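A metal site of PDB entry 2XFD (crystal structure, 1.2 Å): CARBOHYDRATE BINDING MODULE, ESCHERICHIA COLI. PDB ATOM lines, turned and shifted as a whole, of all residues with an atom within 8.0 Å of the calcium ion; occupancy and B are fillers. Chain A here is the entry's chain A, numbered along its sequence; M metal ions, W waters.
The side-chain carboxylate (OE1) of Glu 98 is in hydrogen-bond range of the side-chain amide nitrogen (NE2) of Gln 63, 2.9 Å away. O of Glu 98 is in hydrogen-bond range of N of Val 64 (2.8 Å). The backbone NH (N) of Asp 65 lies within hydrogen-bond range of the backbone carbonyl oxygen (O) of Arg 8 (2.8 Å). O of Asp 65 lies close to N of Ala 76 (3.2 Å).
Four residues have an atom within 4 Å of the calcium ion: Asp 65, Gln 75, Glu 77 and Glu 98.
The side-chain amide oxygen (OE1) of Gln 75 is bound to the calcium ion (2.3 Å). OD1 of Asp 65 binds the calcium ion. OE2 of Glu 98 binds the calcium ion (2.3 Å). The calcium ion is bound by water W1 (2.4 Å). OE2 of Glu 77 is bound to the calcium ion, at 2.5 Å. O of Asp 65 is bound to the calcium ion (2.5 Å). The calcium ion is bound by OE1 of Glu 77. The calcium ion has seven donor atoms within binding distance.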
ATOM      1  N   ARG A   8      -0.267  34.319  30.399  1.00  0.00           N
ATOM      2  CA  ARG A   8      -1.577  34.018  29.824  1.00  0.00           C
ATOM      3  C   ARG A   8      -1.894  32.565  30.180  1.00  0.00           C
ATOM      4  O   ARG A   8      -1.202  31.645  29.748  1.00  0.00           O
ATOM      5  CB  ARG A   8      -1.552  34.220  28.316  1.00  0.00           C
ATOM      6  CG  ARG A   8      -2.961  33.987  27.754  1.00  0.00           C
ATOM      7  CD  ARG A   8      -3.326  34.711  26.613  1.00  0.00           C
ATOM      8  NE  ARG A   8      -4.697  34.649  26.216  1.00  0.00           N
ATOM      9  CZ  ARG A   8      -5.679  35.538  26.431  1.00  0.00           C
ATOM     10  NH1 ARG A   8      -6.842  35.331  25.838  1.00  0.00           N
ATOM     11  NH2 ARG A   8      -5.536  36.572  27.237  1.00  0.00           N
ATOM     12  N   MET A  36      -8.693  31.584  29.226  1.00  0.00           N
ATOM     13  CA  MET A  36      -7.404  32.278  29.154  1.00  0.00           C
ATOM     14  C   MET A  36      -7.550  33.702  29.453  1.00  0.00           C
ATOM     15  O   MET A  36      -8.415  34.407  28.882  1.00  0.00           O
ATOM     16  CB  MET A  36      -6.772  32.101  27.750  1.00  0.00           C
ATOM     17  CG  MET A  36      -6.304  30.708  27.412  1.00  0.00           C
ATOM     18  SD  MET A  36      -4.929  30.240  28.447  1.00  0.00           S
ATOM     19  CE  MET A  36      -4.636  28.612  27.839  1.00  0.00           C
ATOM     20  N   GLN A  63      -3.604  25.283  32.286  1.00  0.00           N
ATOM     21  CA  GLN A  63      -3.096  25.401  30.909  1.00  0.00           C
ATOM     22  C   GLN A  63      -2.482  26.815  30.805  1.00  0.00           C
ATOM     23  O   GLN A  63      -3.194  27.798  30.922  1.00  0.00           O
ATOM     24  CB  GLN A  63      -4.179  25.169  29.883  1.00  0.00           C
ATOM     25  CG  GLN A  63      -3.673  25.118  28.457  1.00  0.00           C
ATOM     26  CD  GLN A  63      -4.746  25.092  27.404  1.00  0.00           C
ATOM     27  OE1 GLN A  63      -5.931  25.263  27.662  1.00  0.00           O
ATOM     28  NE2 GLN A  63      -4.374  24.835  26.221  1.00  0.00           N
ATOM     29  N   VAL A  64      -1.174  26.869  30.550  1.00  0.00           N
ATOM     30  CA  VAL A  64      -0.445  28.116  30.329  1.00  0.00           C
ATOM     31  C   VAL A  64      -0.199  28.252  28.864  1.00  0.00           C
ATOM     32  O   VAL A  64       0.457  27.422  28.261  1.00  0.00           O
ATOM     33  CB  VAL A  64       0.906  28.103  31.141  1.00  0.00           C
ATOM     34  CG1 VAL A  64       1.603  29.445  30.922  1.00  0.00           C
ATOM     35  CG2 VAL A  64       0.728  27.784  32.569  1.00  0.00           C
ATOM     36  N   ASP A  65      -0.741  29.276  28.265  1.00  0.00           N
ATOM     37  CA  ASP A  65      -0.514  29.510  26.851  1.00  0.00           C
ATOM     38  C   ASP A  65       0.926  29.941  26.579  1.00  0.00           C
ATOM     39  O   ASP A  65       1.666  29.329  25.759  1.00  0.00           O
ATOM     40  CB  ASP A  65      -1.518  30.521  26.259  1.00  0.00           C
ATOM     41  CG  ASP A  65      -1.554  30.565  24.757  1.00  0.00           C
ATOM     42  OD1 ASP A  65      -0.738  29.948  24.104  1.00  0.00           O
ATOM     43  OD2 ASP A  65      -2.462  31.259  24.232  1.00  0.00           O
ATOM     44  N   TYR A  66       1.357  30.975  27.259  1.00  0.00           N
ATOM     45  CA  TYR A  66       2.608  31.636  27.047  1.00  0.00           C
ATOM     46  C   TYR A  66       2.829  32.610  28.194  1.00  0.00           C
ATOM     47  O   TYR A  66       1.907  32.933  28.947  1.00  0.00           O
ATOM     48  CB  TYR A  66       2.712  32.342  25.663  1.00  0.00           C
ATOM     49  CG  TYR A  66       1.633  33.377  25.421  1.00  0.00           C
ATOM     50  CD1 TYR A  66       1.654  34.604  26.005  1.00  0.00           C
ATOM     51  CD2 TYR A  66       0.604  33.115  24.550  1.00  0.00           C
ATOM     52  CE1 TYR A  66       0.701  35.583  25.721  1.00  0.00           C
ATOM     53  CE2 TYR A  66      -0.362  34.051  24.280  1.00  0.00           C
ATOM     54  CZ  TYR A  66      -0.312  35.277  24.873  1.00  0.00           C
ATOM     55  OH  TYR A  66      -1.315  36.212  24.599  1.00  0.00           O
ATOM     56  N   ILE A  67       4.055  33.142  28.257  1.00  0.00           N
ATOM     57  CA  ILE A  67       4.315  34.360  28.980  1.00  0.00           C
ATOM     58  C   ILE A  67       4.885  35.368  27.994  1.00  0.00           C
ATOM     59  O   ILE A  67       5.341  35.039  26.902  1.00  0.00           O
ATOM     60  CB  ILE A  67       5.254  34.167  30.219  1.00  0.00           C
ATOM     61  CG1 ILE A  67       6.698  33.940  29.811  1.00  0.00           C
ATOM     62  CG2 ILE A  67       4.703  33.070  31.090  1.00  0.00           C
ATOM     63  CD1 ILE A  67       7.635  33.903  30.990  1.00  0.00           C
ATOM     64  N   THR A  73       7.196  37.209  23.590  1.00  0.00           N
ATOM     65  CA  THR A  73       6.355  36.047  23.878  1.00  0.00           C
ATOM     66  C   THR A  73       7.205  34.793  23.942  1.00  0.00           C
ATOM     67  O   THR A  73       7.979  34.549  22.996  1.00  0.00           O
ATOM     68  CB  THR A  73       5.236  35.924  22.856  1.00  0.00           C
ATOM     69  OG1 THR A  73       4.350  37.041  22.953  1.00  0.00           O
ATOM     70  CG2 THR A  73       4.404  34.687  23.019  1.00  0.00           C
ATOM     71  N   ARG A  74       7.046  33.991  24.971  1.00  0.00           N
ATOM     72  CA  ARG A  74       7.724  32.726  25.148  1.00  0.00           C
ATOM     73  C   ARG A  74       6.634  31.681  25.351  1.00  0.00           C
ATOM     74  O   ARG A  74       5.950  31.693  26.383  1.00  0.00           O
ATOM     75  CB  ARG A  74       8.687  32.812  26.346  1.00  0.00           C
ATOM     76  CG  ARG A  74       9.716  33.927  26.255  1.00  0.00           C
ATOM     77  CD  ARG A  74      10.642  33.871  27.399  1.00  0.00           C
ATOM     78  NE  ARG A  74      11.558  35.006  27.422  1.00  0.00           N
ATOM     79  CZ  ARG A  74      12.435  35.246  28.372  1.00  0.00           C
ATOM     80  NH1 ARG A  74      12.611  34.425  29.379  1.00  0.00           N
ATOM     81  NH2 ARG A  74      13.139  36.399  28.338  1.00  0.00           N
ATOM     82  N   GLN A  75       6.405  30.842  24.369  1.00  0.00           N
ATOM     83  CA  GLN A  75       5.333  29.852  24.436  1.00  0.00           C
ATOM     84  C   GLN A  75       5.625  28.804  25.493  1.00  0.00           C
ATOM     85  O   GLN A  75       6.737  28.272  25.540  1.00  0.00           O
ATOM     86  CB  GLN A  75       5.168  29.183  23.121  1.00  0.00           C
ATOM     87  CG  GLN A  75       4.686  30.061  21.971  1.00  0.00           C
ATOM     88  CD  GLN A  75       3.274  30.548  22.134  1.00  0.00           C
ATOM     89  OE1 GLN A  75       2.476  29.991  22.861  1.00  0.00           O
ATOM     90  NE2 GLN A  75       2.944  31.649  21.449  1.00  0.00           N
ATOM     91  N   ALA A  76       4.632  28.406  26.290  1.00  0.00           N
ATOM     92  CA  ALA A  76       4.866  27.346  27.272  1.00  0.00           C
ATOM     93  C   ALA A  76       5.315  26.051  26.643  1.00  0.00           C
ATOM     94  O   ALA A  76       6.196  25.365  27.167  1.00  0.00           O
ATOM     95  CB  ALA A  76       3.590  27.178  28.107  1.00  0.00           C
ATOM     96  N   GLU A  77       4.702  25.688  25.507  1.00  0.00           N
ATOM     97  CA  GLU A  77       4.993  24.465  24.801  1.00  0.00           C
ATOM     98  C   GLU A  77       6.373  24.448  24.158  1.00  0.00           C
ATOM     99  O   GLU A  77       6.828  23.399  23.727  1.00  0.00           O
ATOM    100  CB  GLU A  77       3.887  24.154  23.770  1.00  0.00           C
ATOM    101  CG  GLU A  77       3.703  25.204  22.650  1.00  0.00           C
ATOM    102  CD  GLU A  77       2.742  26.317  22.986  1.00  0.00           C
ATOM    103  OE1 GLU A  77       2.026  26.768  22.055  1.00  0.00           O
ATOM    104  OE2 GLU A  77       2.714  26.812  24.129  1.00  0.00           O
ATOM    105  N   ASN A  78       7.030  25.610  24.084  1.00  0.00           N
ATOM    106  CA  ASN A  78       8.412  25.688  23.600  1.00  0.00           C
ATOM    107  C   ASN A  78       9.440  25.539  24.698  1.00  0.00           C
ATOM    108  O   ASN A  78      10.627  25.598  24.394  1.00  0.00           O
ATOM    109  CB  ASN A  78       8.629  26.997  22.793  1.00  0.00           C
ATOM    110  CG  ASN A  78       7.825  27.034  21.505  1.00  0.00           C
ATOM    111  OD1 ASN A  78       7.291  26.004  21.062  1.00  0.00           O
ATOM    112  ND2 ASN A  78       7.738  28.175  20.886  1.00  0.00           N
ATOM    113  N   SER A  97       5.057  21.359  27.013  1.00  0.00           N
ATOM    114  CA  SER A  97       3.594  21.304  27.149  1.00  0.00           C
ATOM    115  C   SER A  97       3.112  22.597  27.828  1.00  0.00           C
ATOM    116  O   SER A  97       3.771  23.162  28.687  1.00  0.00           O
ATOM    117  CB  SER A  97       3.183  20.127  28.011  1.00  0.00           C
ATOM    118  OG  SER A  97       1.788  20.090  28.200  1.00  0.00           O
ATOM    119  N   GLU A  98       1.919  23.021  27.415  1.00  0.00           N
ATOM    120  CA  GLU A  98       1.161  24.049  28.090  1.00  0.00           C
ATOM    121  C   GLU A  98       0.629  23.634  29.429  1.00  0.00           C
ATOM    122  O   GLU A  98       0.197  24.466  30.219  1.00  0.00           O
ATOM    123  CB  GLU A  98       0.010  24.510  27.210  1.00  0.00           C
ATOM    124  CG  GLU A  98       0.459  25.216  25.950  1.00  0.00           C
ATOM    125  CD  GLU A  98      -0.661  25.735  25.078  1.00  0.00           C
ATOM    126  OE1 GLU A  98      -1.720  25.046  25.030  1.00  0.00           O
ATOM    127  OE2 GLU A  98      -0.497  26.765  24.415  1.00  0.00           O
HETATM  128 CA    CA M   1       0.933  28.415  23.588  1.00  0.00          CA
HETATM  129  O   HOH W   1      -0.266  28.730  21.560  1.00  0.00           O
